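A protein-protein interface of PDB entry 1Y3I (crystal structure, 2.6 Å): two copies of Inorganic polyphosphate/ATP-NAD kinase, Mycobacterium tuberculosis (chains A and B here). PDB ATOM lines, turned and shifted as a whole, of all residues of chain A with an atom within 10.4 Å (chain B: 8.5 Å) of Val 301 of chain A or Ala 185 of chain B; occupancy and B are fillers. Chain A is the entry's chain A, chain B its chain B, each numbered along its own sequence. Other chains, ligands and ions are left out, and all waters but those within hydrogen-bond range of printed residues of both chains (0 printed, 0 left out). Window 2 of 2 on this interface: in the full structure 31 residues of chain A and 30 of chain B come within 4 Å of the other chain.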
ATOM      1  N   THR A 290      14.992   1.817   9.459  1.00  0.00           N
ATOM      2  CA  THR A 290      15.055   2.449   8.142  1.00  0.00           C
ATOM      3  C   THR A 290      16.469   2.867   7.760  1.00  0.00           C
ATOM      4  O   THR A 290      16.773   3.041   6.579  1.00  0.00           O
ATOM      5  CB  THR A 290      14.115   3.668   8.114  1.00  0.00           C
ATOM      6  OG1 THR A 290      12.875   3.281   8.724  1.00  0.00           O
ATOM      7  CG2 THR A 290      13.825   4.085   6.685  1.00  0.00           C
ATOM      8  N   ASP A 291      17.338   3.028   8.750  1.00  0.00           N
ATOM      9  CA  ASP A 291      18.741   3.341   8.534  1.00  0.00           C
ATOM     10  C   ASP A 291      19.532   2.116   8.095  1.00  0.00           C
ATOM     11  O   ASP A 291      20.394   2.210   7.220  1.00  0.00           O
ATOM     12  CB  ASP A 291      19.325   3.936   9.818  1.00  0.00           C
ATOM     13  CG  ASP A 291      19.381   5.450   9.764  1.00  0.00           C
ATOM     14  OD1 ASP A 291      18.528   6.066   9.095  1.00  0.00           O
ATOM     15  OD2 ASP A 291      20.299   6.017  10.398  1.00  0.00           O
ATOM     16  N   LEU A 293      18.136  -0.731   6.603  1.00  0.00           N
ATOM     17  CA  LEU A 293      17.436  -0.983   5.351  1.00  0.00           C
ATOM     18  C   LEU A 293      17.917  -0.086   4.220  1.00  0.00           C
ATOM     19  O   LEU A 293      18.107  -0.526   3.087  1.00  0.00           O
ATOM     20  CB  LEU A 293      15.930  -0.803   5.581  1.00  0.00           C
ATOM     21  CG  LEU A 293      15.085  -0.490   4.347  1.00  0.00           C
ATOM     22  CD1 LEU A 293      14.987  -1.724   3.462  1.00  0.00           C
ATOM     23  CD2 LEU A 293      13.728   0.036   4.780  1.00  0.00           C
ATOM     24  N   VAL A 294      18.128   1.196   4.500  1.00  0.00           N
ATOM     25  CA  VAL A 294      18.537   2.115   3.446  1.00  0.00           C
ATOM     26  C   VAL A 294      19.940   1.812   2.936  1.00  0.00           C
ATOM     27  O   VAL A 294      20.135   1.694   1.726  1.00  0.00           O
ATOM     28  CB  VAL A 294      18.495   3.589   3.901  1.00  0.00           C
ATOM     29  CG1 VAL A 294      19.137   3.770   5.269  1.00  0.00           C
ATOM     30  CG2 VAL A 294      19.188   4.485   2.882  1.00  0.00           C
ATOM     31  N   ARG A 295      20.910   1.709   3.837  1.00  0.00           N
ATOM     32  CA  ARG A 295      22.302   1.542   3.410  1.00  0.00           C
ATOM     33  C   ARG A 295      22.525   0.142   2.861  1.00  0.00           C
ATOM     34  O   ARG A 295      23.076  -0.037   1.774  1.00  0.00           O
ATOM     35  CB  ARG A 295      23.263   1.849   4.557  1.00  0.00           C
ATOM     36  CG  ARG A 295      24.275   0.772   4.887  1.00  0.00           C
ATOM     37  CD  ARG A 295      25.525   0.851   4.027  1.00  0.00           C
ATOM     38  NE  ARG A 295      26.255  -0.413   4.005  1.00  0.00           N
ATOM     39  CZ  ARG A 295      26.055  -1.431   3.182  1.00  0.00           C
ATOM     40  NH1 ARG A 295      26.813  -2.518   3.299  1.00  0.00           N
ATOM     41  NH2 ARG A 295      25.118  -1.393   2.247  1.00  0.00           N
ATOM     42  N   PHE A 297      20.546  -2.000   1.657  1.00  0.00           N
ATOM     43  CA  PHE A 297      19.819  -2.147   0.410  1.00  0.00           C
ATOM     44  C   PHE A 297      20.206  -1.056  -0.585  1.00  0.00           C
ATOM     45  O   PHE A 297      20.031  -1.191  -1.797  1.00  0.00           O
ATOM     46  CB  PHE A 297      18.318  -2.068   0.694  1.00  0.00           C
ATOM     47  CG  PHE A 297      17.635  -3.417   0.800  1.00  0.00           C
ATOM     48  CD1 PHE A 297      18.378  -4.578   0.699  1.00  0.00           C
ATOM     49  CD2 PHE A 297      16.265  -3.486   0.996  1.00  0.00           C
ATOM     50  CE1 PHE A 297      17.762  -5.814   0.789  1.00  0.00           C
ATOM     51  CE2 PHE A 297      15.649  -4.718   1.084  1.00  0.00           C
ATOM     52  CZ  PHE A 297      16.397  -5.876   0.985  1.00  0.00           C
ATOM     53  N   ARG A 298      20.723   0.049  -0.053  1.00  0.00           N
ATOM     54  CA  ARG A 298      21.045   1.207  -0.875  1.00  0.00           C
ATOM     55  C   ARG A 298      19.821   1.690  -1.651  1.00  0.00           C
ATOM     56  O   ARG A 298      19.855   1.724  -2.881  1.00  0.00           O
ATOM     57  CB  ARG A 298      22.196   0.867  -1.826  1.00  0.00           C
ATOM     58  CG  ARG A 298      23.460   0.421  -1.103  1.00  0.00           C
ATOM     59  CD  ARG A 298      24.639   1.350  -1.320  1.00  0.00           C
ATOM     60  NE  ARG A 298      25.296   1.763  -0.080  1.00  0.00           N
ATOM     61  CZ  ARG A 298      26.425   1.239   0.384  1.00  0.00           C
ATOM     62  NH1 ARG A 298      27.037   0.270  -0.289  1.00  0.00           N
ATOM     63  NH2 ARG A 298      26.947   1.679   1.519  1.00  0.00           N
ATOM     64  N   LEU A 299      18.774   2.042  -0.920  1.00  0.00           N
ATOM     65  CA  LEU A 299      17.488   2.487  -1.426  1.00  0.00           C
ATOM     66  C   LEU A 299      17.566   3.809  -2.178  1.00  0.00           C
ATOM     67  O   LEU A 299      18.026   4.818  -1.636  1.00  0.00           O
ATOM     68  CB  LEU A 299      16.492   2.638  -0.265  1.00  0.00           C
ATOM     69  CG  LEU A 299      16.019   1.331   0.371  1.00  0.00           C
ATOM     70  CD1 LEU A 299      15.031   1.598   1.494  1.00  0.00           C
ATOM     71  CD2 LEU A 299      15.406   0.424  -0.684  1.00  0.00           C
ATOM     72  N   PRO A 300      17.111   3.825  -3.421  1.00  0.00           N
ATOM     73  CA  PRO A 300      17.199   5.059  -4.207  1.00  0.00           C
ATOM     74  C   PRO A 300      16.104   6.019  -3.752  1.00  0.00           C
ATOM     75  O   PRO A 300      14.976   5.973  -4.234  1.00  0.00           O
ATOM     76  CB  PRO A 300      16.976   4.613  -5.647  1.00  0.00           C
ATOM     77  CG  PRO A 300      16.881   3.125  -5.612  1.00  0.00           C
ATOM     78  CD  PRO A 300      16.476   2.763  -4.208  1.00  0.00           C
ATOM     79  N   VAL A 301      16.464   6.887  -2.816  1.00  0.00           N
ATOM     80  CA  VAL A 301      15.548   7.965  -2.429  1.00  0.00           C
ATOM     81  C   VAL A 301      15.853   9.199  -3.285  1.00  0.00           C
ATOM     82  O   VAL A 301      15.525  10.339  -2.963  1.00  0.00           O
ATOM     83  CB  VAL A 301      15.636   8.260  -0.929  1.00  0.00           C
ATOM     84  CG1 VAL A 301      15.956   6.970  -0.182  1.00  0.00           C
ATOM     85  CG2 VAL A 301      16.680   9.326  -0.630  1.00  0.00           C
ATOM     86  N   THR A 302      16.492   8.894  -4.398  1.00  0.00           N
ATOM     87  CA  THR A 302      16.804   9.728  -5.537  1.00  0.00           C
ATOM     88  C   THR A 302      15.536  10.280  -6.174  1.00  0.00           C
ATOM     89  O   THR A 302      14.809  11.041  -5.505  1.00  0.00           O
ATOM     90  CB  THR A 302      17.604   8.928  -6.587  1.00  0.00           C
ATOM     91  OG1 THR A 302      16.801   7.884  -7.158  1.00  0.00           O
ATOM     92  CG2 THR A 302      18.797   8.252  -5.923  1.00  0.00           C
ATOM     93  N   LEU B 172       2.414  12.936  -8.953  1.00  0.00           N
ATOM     94  CA  LEU B 172       2.536  13.681  -7.715  1.00  0.00           C
ATOM     95  C   LEU B 172       3.806  13.281  -6.948  1.00  0.00           C
ATOM     96  O   LEU B 172       4.002  12.096  -6.692  1.00  0.00           O
ATOM     97  CB  LEU B 172       1.354  13.489  -6.761  1.00  0.00           C
ATOM     98  CG  LEU B 172       1.642  13.847  -5.294  1.00  0.00           C
ATOM     99  CD1 LEU B 172       1.937  15.336  -5.172  1.00  0.00           C
ATOM    100  CD2 LEU B 172       0.496  13.456  -4.384  1.00  0.00           C
ATOM    101  N   GLY B 173       4.561  14.320  -6.615  1.00  0.00           N
ATOM    102  CA  GLY B 173       5.835  14.239  -5.933  1.00  0.00           C
ATOM    103  C   GLY B 173       5.633  13.970  -4.459  1.00  0.00           C
ATOM    104  O   GLY B 173       4.789  14.606  -3.832  1.00  0.00           O
ATOM    105  N   VAL B 174       6.393  13.031  -3.906  1.00  0.00           N
ATOM    106  CA  VAL B 174       6.072  12.574  -2.560  1.00  0.00           C
ATOM    107  C   VAL B 174       7.250  11.914  -1.878  1.00  0.00           C
ATOM    108  O   VAL B 174       8.004  11.181  -2.530  1.00  0.00           O
ATOM    109  CB  VAL B 174       4.921  11.548  -2.658  1.00  0.00           C
ATOM    110  CG1 VAL B 174       5.153  10.402  -1.686  1.00  0.00           C
ATOM    111  CG2 VAL B 174       3.572  12.207  -2.422  1.00  0.00           C
ATOM    112  N   VAL B 175       7.436  12.144  -0.577  1.00  0.00           N
ATOM    113  CA  VAL B 175       8.524  11.449   0.106  1.00  0.00           C
ATOM    114  C   VAL B 175       7.979  10.639   1.286  1.00  0.00           C
ATOM    115  O   VAL B 175       7.322  11.177   2.172  1.00  0.00           O
ATOM    116  CB  VAL B 175       9.648  12.324   0.680  1.00  0.00           C
ATOM    117  CG1 VAL B 175      10.184  11.683   1.953  1.00  0.00           C
ATOM    118  CG2 VAL B 175      10.770  12.497  -0.323  1.00  0.00           C
ATOM    119  N   VAL B 176       8.320   9.357   1.217  1.00  0.00           N
ATOM    120  CA  VAL B 176       7.966   8.451   2.300  1.00  0.00           C
ATOM    121  C   VAL B 176       9.203   8.304   3.193  1.00  0.00           C
ATOM    122  O   VAL B 176      10.237   7.841   2.717  1.00  0.00           O
ATOM    123  CB  VAL B 176       7.488   7.075   1.826  1.00  0.00           C
ATOM    124  CG1 VAL B 176       7.449   6.097   2.992  1.00  0.00           C
ATOM    125  CG2 VAL B 176       6.118   7.152   1.166  1.00  0.00           C
ATOM    126  N   GLU B 177       9.013   8.743   4.425  1.00  0.00           N
ATOM    127  CA  GLU B 177       9.914   8.613   5.549  1.00  0.00           C
ATOM    128  C   GLU B 177       9.242   7.719   6.603  1.00  0.00           C
ATOM    129  O   GLU B 177       8.082   7.926   6.970  1.00  0.00           O
ATOM    130  CB  GLU B 177      10.305   9.925   6.216  1.00  0.00           C
ATOM    131  CG  GLU B 177      10.740  11.075   5.340  1.00  0.00           C
ATOM    132  CD  GLU B 177      11.115  12.334   6.101  1.00  0.00           C
ATOM    133  OE1 GLU B 177      10.862  12.395   7.326  1.00  0.00           O
ATOM    134  OE2 GLU B 177      11.668  13.271   5.472  1.00  0.00           O
ATOM    135  N   ARG B 181      13.416   8.450   8.822  1.00  0.00           N
ATOM    136  CA  ARG B 181      14.333   8.320   7.683  1.00  0.00           C
ATOM    137  C   ARG B 181      13.497   8.224   6.409  1.00  0.00           C
ATOM    138  O   ARG B 181      12.583   7.399   6.359  1.00  0.00           O
ATOM    139  CB  ARG B 181      15.263   7.130   7.819  1.00  0.00           C
ATOM    140  CG  ARG B 181      15.874   6.951   9.190  1.00  0.00           C
ATOM    141  CD  ARG B 181      16.439   8.246   9.759  1.00  0.00           C
ATOM    142  NE  ARG B 181      17.378   8.012  10.846  1.00  0.00           N
ATOM    143  CZ  ARG B 181      17.263   8.315  12.132  1.00  0.00           C
ATOM    144  NH1 ARG B 181      16.170   8.908  12.601  1.00  0.00           N
ATOM    145  NH2 ARG B 181      18.245   8.016  12.972  1.00  0.00           N
ATOM    146  N   PRO B 182      13.791   9.050   5.414  1.00  0.00           N
ATOM    147  CA  PRO B 182      13.020   9.003   4.163  1.00  0.00           C
ATOM    148  C   PRO B 182      13.444   7.771   3.367  1.00  0.00           C
ATOM    149  O   PRO B 182      14.567   7.721   2.866  1.00  0.00           O
ATOM    150  CB  PRO B 182      13.416  10.294   3.460  1.00  0.00           C
ATOM    151  CG  PRO B 182      14.801  10.564   3.946  1.00  0.00           C
ATOM    152  CD  PRO B 182      14.847  10.066   5.362  1.00  0.00           C
ATOM    153  N   VAL B 183      12.535   6.816   3.296  1.00  0.00           N
ATOM    154  CA  VAL B 183      12.739   5.487   2.753  1.00  0.00           C
ATOM    155  C   VAL B 183      12.527   5.447   1.246  1.00  0.00           C
ATOM    156  O   VAL B 183      13.028   4.592   0.512  1.00  0.00           O
ATOM    157  CB  VAL B 183      11.775   4.491   3.430  1.00  0.00           C
ATOM    158  CG1 VAL B 183      10.589   4.194   2.528  1.00  0.00           C
ATOM    159  CG2 VAL B 183      12.502   3.207   3.798  1.00  0.00           C
ATOM    160  N   SER B 184      11.754   6.435   0.783  1.00  0.00           N
ATOM    161  CA  SER B 184      11.492   6.450  -0.651  1.00  0.00           C
ATOM    162  C   SER B 184      10.898   7.769  -1.108  1.00  0.00           C
ATOM    163  O   SER B 184      10.045   8.383  -0.474  1.00  0.00           O
ATOM    164  CB  SER B 184      10.561   5.286  -0.991  1.00  0.00           C
ATOM    165  OG  SER B 184       9.284   5.445  -0.401  1.00  0.00           O
ATOM    166  N   ALA B 185      11.388   8.200  -2.269  1.00  0.00           N
ATOM    167  CA  ALA B 185      10.768   9.356  -2.904  1.00  0.00           C
ATOM    168  C   ALA B 185      10.406   9.019  -4.347  1.00  0.00           C
ATOM    169  O   ALA B 185      11.156   8.326  -5.040  1.00  0.00           O
ATOM    170  CB  ALA B 185      11.690  10.553  -2.820  1.00  0.00           C
ATOM    171  N   PHE B 186       9.249   9.510  -4.799  1.00  0.00           N
ATOM    172  CA  PHE B 186       8.884   9.303  -6.194  1.00  0.00           C
ATOM    173  C   PHE B 186       7.663  10.111  -6.630  1.00  0.00           C
ATOM    174  O   PHE B 186       6.967  10.710  -5.816  1.00  0.00           O
ATOM    175  CB  PHE B 186       8.611   7.822  -6.450  1.00  0.00           C
ATOM    176  CG  PHE B 186       7.746   7.103  -5.439  1.00  0.00           C
ATOM    177  CD1 PHE B 186       6.407   7.395  -5.275  1.00  0.00           C
ATOM    178  CD2 PHE B 186       8.310   6.108  -4.657  1.00  0.00           C
ATOM    179  CE1 PHE B 186       5.626   6.726  -4.357  1.00  0.00           C
ATOM    180  CE2 PHE B 186       7.550   5.438  -3.723  1.00  0.00           C
ATOM    181  CZ  PHE B 186       6.217   5.757  -3.567  1.00  0.00           C
ATOM    182  N   GLY B 187       7.443  10.043  -7.940  1.00  0.00           N
ATOM    183  CA  GLY B 187       6.256  10.587  -8.583  1.00  0.00           C
ATOM    184  C   GLY B 187       5.182   9.521  -8.576  1.00  0.00           C
ATOM    185  O   GLY B 187       5.483   8.353  -8.851  1.00  0.00           O
ATOM    186  N   CYS B 188       3.932   9.856  -8.249  1.00  0.00           N
ATOM    187  CA  CYS B 188       3.056   8.687  -8.122  1.00  0.00           C
ATOM    188  C   CYS B 188       1.593   9.066  -8.079  1.00  0.00           C
ATOM    189  O   CYS B 188       1.255  10.232  -7.893  1.00  0.00           O
ATOM    190  CB  CYS B 188       3.451   7.954  -6.831  1.00  0.00           C
ATOM    191  SG  CYS B 188       3.610   9.134  -5.462  1.00  0.00           S
ATOM    192  N   VAL B 191      -0.135   7.468  -2.155  1.00  0.00           N
ATOM    193  CA  VAL B 191       0.420   6.449  -1.259  1.00  0.00           C
ATOM    194  C   VAL B 191      -0.669   5.838  -0.373  1.00  0.00           C
ATOM    195  O   VAL B 191      -1.540   6.482   0.212  1.00  0.00           O
ATOM    196  CB  VAL B 191       1.567   6.942  -0.365  1.00  0.00           C
ATOM    197  CG1 VAL B 191       2.140   5.754   0.396  1.00  0.00           C
ATOM    198  CG2 VAL B 191       2.683   7.621  -1.135  1.00  0.00           C
ATOM    199  N   ALA B 225       3.943   4.284  -8.715  1.00  0.00           N
ATOM    200  CA  ALA B 225       5.132   5.099  -8.528  1.00  0.00           C
ATOM    201  C   ALA B 225       6.069   5.047  -9.722  1.00  0.00           C
ATOM    202  O   ALA B 225       6.548   3.979 -10.114  1.00  0.00           O
ATOM    203  CB  ALA B 225       5.853   4.632  -7.268  1.00  0.00           C
ATOM    204  N   HIS B 226       6.359   6.210 -10.316  1.00  0.00           N
ATOM    205  CA  HIS B 226       7.396   6.178 -11.356  1.00  0.00           C
ATOM    206  C   HIS B 226       8.756   6.054 -10.663  1.00  0.00           C
ATOM    207  O   HIS B 226       9.509   7.026 -10.581  1.00  0.00           O
ATOM    208  CB  HIS B 226       7.350   7.396 -12.269  1.00  0.00           C
ATOM    209  CG  HIS B 226       7.802   7.159 -13.679  1.00  0.00           C
ATOM    210  ND1 HIS B 226       9.073   7.409 -14.145  1.00  0.00           N
ATOM    211  CD2 HIS B 226       7.124   6.686 -14.751  1.00  0.00           C
ATOM    212  CE1 HIS B 226       9.159   7.098 -15.426  1.00  0.00           C
ATOM    213  NE2 HIS B 226       7.983   6.655 -15.824  1.00  0.00           N
ATOM    214  N   ALA B 227       9.038   4.857 -10.156  1.00  0.00           N
ATOM    215  CA  ALA B 227      10.261   4.583  -9.418  1.00  0.00           C
ATOM    216  C   ALA B 227      10.721   3.133  -9.574  1.00  0.00           C
ATOM    217  O   ALA B 227       9.907   2.247  -9.830  1.00  0.00           O
ATOM    218  CB  ALA B 227      10.088   4.878  -7.934  1.00  0.00           C
ATOM    219  N   LEU B 228      12.024   2.950  -9.398  1.00  0.00           N
ATOM    220  CA  LEU B 228      12.704   1.678  -9.510  1.00  0.00           C
ATOM    221  C   LEU B 228      12.332   0.730  -8.371  1.00  0.00           C
ATOM    222  O   LEU B 228      12.338  -0.482  -8.575  1.00  0.00           O
ATOM    223  CB  LEU B 228      14.222   1.866  -9.471  1.00  0.00           C
ATOM    224  CG  LEU B 228      14.921   1.939 -10.828  1.00  0.00           C
ATOM    225  CD1 LEU B 228      15.673   0.642 -11.108  1.00  0.00           C
ATOM    226  CD2 LEU B 228      13.916   2.241 -11.931  1.00  0.00           C
ATOM    227  N   PHE B 229      12.045   1.360  -7.234  1.00  0.00           N
ATOM    228  CA  PHE B 229      11.743   0.605  -6.024  1.00  0.00           C
ATOM    229  C   PHE B 229      10.499   1.132  -5.317  1.00  0.00           C
ATOM    230  O   PHE B 229      10.474   2.272  -4.864  1.00  0.00           O
ATOM    231  CB  PHE B 229      12.950   0.625  -5.083  1.00  0.00           C
ATOM    232  CG  PHE B 229      12.782  -0.304  -3.891  1.00  0.00           C
ATOM    233  CD1 PHE B 229      12.855  -1.677  -4.040  1.00  0.00           C
ATOM    234  CD2 PHE B 229      12.552   0.213  -2.626  1.00  0.00           C
ATOM    235  CE1 PHE B 229      12.697  -2.519  -2.956  1.00  0.00           C
ATOM    236  CE2 PHE B 229      12.395  -0.623  -1.538  1.00  0.00           C
ATOM    237  CZ  PHE B 229      12.474  -1.995  -1.697  1.00  0.00           C
ATOM    238  N   GLY B 230       9.498   0.264  -5.257  1.00  0.00           N
ATOM    239  CA  GLY B 230       8.213   0.515  -4.636  1.00  0.00           C
ATOM    240  C   GLY B 230       7.715  -0.725  -3.909  1.00  0.00           C
ATOM    241  O   GLY B 230       6.523  -0.914  -3.681  1.00  0.00           O
ATOM    242  N   MET B 233       6.383  -2.198   2.055  1.00  0.00           N
ATOM    243  CA  MET B 233       7.082  -2.283   3.333  1.00  0.00           C
ATOM    244  C   MET B 233       6.091  -2.499   4.477  1.00  0.00           C
ATOM    245  O   MET B 233       5.128  -1.727   4.612  1.00  0.00           O
ATOM    246  CB  MET B 233       7.897  -1.007   3.555  1.00  0.00           C
ATOM    247  CG  MET B 233       9.205  -0.911   2.782  1.00  0.00           C
ATOM    248  SD  MET B 233       9.592   0.823   2.400  1.00  0.00           S
ATOM    249  CE  MET B 233      11.235   0.617   1.719  1.00  0.00           C
ATOM    250  N   GLU B 244       5.926  13.326   2.433  1.00  0.00           N
ATOM    251  CA  GLU B 244       6.107  14.761   2.236  1.00  0.00           C
ATOM    252  C   GLU B 244       5.673  15.203   0.842  1.00  0.00           C
ATOM    253  O   GLU B 244       6.247  14.742  -0.146  1.00  0.00           O
ATOM    254  CB  GLU B 244       7.568  15.139   2.459  1.00  0.00           C
ATOM    255  CG  GLU B 244       7.724  16.601   2.878  1.00  0.00           C
ATOM    256  CD  GLU B 244       8.250  16.694   4.299  1.00  0.00           C
ATOM    257  OE1 GLU B 244       7.579  17.326   5.143  1.00  0.00           O
ATOM    258  OE2 GLU B 244       9.332  16.119   4.544  1.00  0.00           O
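The side-chain carboxylate (OD1) of Asp 291 of chain A lies within salt-bridge range of the guanidinium group (NE) of Arg 181 of chain B.
The backbone carbonyl oxygen (O) of Val 294 of chain A sits at hydrogen-bond distance from the backbone NH (N) of Leu 299 of chain A.
The backbone carbonyl oxygen of Val 176 of chain B lies within hydrogen-bond range of the backbone NH of Val 183 of chain B (2.6 Å).
Among the printed residues, merely in contact across the chains: Thr 290 of chain A with Arg 181 of chain B (3.6 Å), Thr 290 of chain A with Val 183 of chain B (3.3 Å), Leu 293 of chain A with Val 183 of chain B (3.5 Å), Leu 293 of chain A with Met 233 of chain B (3.99 Å), Leu 299 of chain A with Val 183 of chain B (3.7 Å), Leu 299 of chain A with Phe 229 of chain B (3.3 Å), Leu 299 of chain A with Met 233 of chain B (3.9 Å), Val 301 of chain A with Pro 182 of chain B (3.4 Å), Val 301 of chain A with Val 183 of chain B (3.8 Å) and Val 301 of chain A with Ala 185 of chain B (3.8 Å).
Of chain B, only Pro 182 (3.4 Å), Val 183 (3.8 Å) and Ala 185 (3.8 Å) come within 4 Å of Val 301 of chain A.
No residue of chain B comes within 4 Å of Thr 302 of chain A.
Gly 173 of chain B touches none of the printed residues of chain A.
Of the printed residues of chain A, Pro 182 of chain B touches Val 301 (3.4 Å).
No residue of chain A comes within 4 Å of Ser 184 of chain B.
Of chain A, only Val 301 (3.8 Å) comes within 4 Å of Ala 185 of chain B.
Of the printed residues of chain A, Phe 229 of chain B touches Leu 299.
The nearest residue of chain B that does not touch Val 301 of chain A is Ser 184 of chain B (4.3 Å).
The nearest printed residue of chain A that does not touch Arg 181 of chain B is Val 294 of chain A (5.7 Å).
Hydrophobic or aromatic side chains of chain A that line the printed part of chain B: Leu 293, Leu 299 and Val 301.
Of the 23 printed residues of chain B, 6 touch a printed residue of chain A.
Among the printed residues, 11 pairs touch across the chains.
Among the printed residues, Asp or Glu carboxylates within 4 Å of a Lys or Arg side-chain nitrogen of the other chain: Asp 291 of chain A with Arg 181 of chain B.
No position is printed for both chains.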
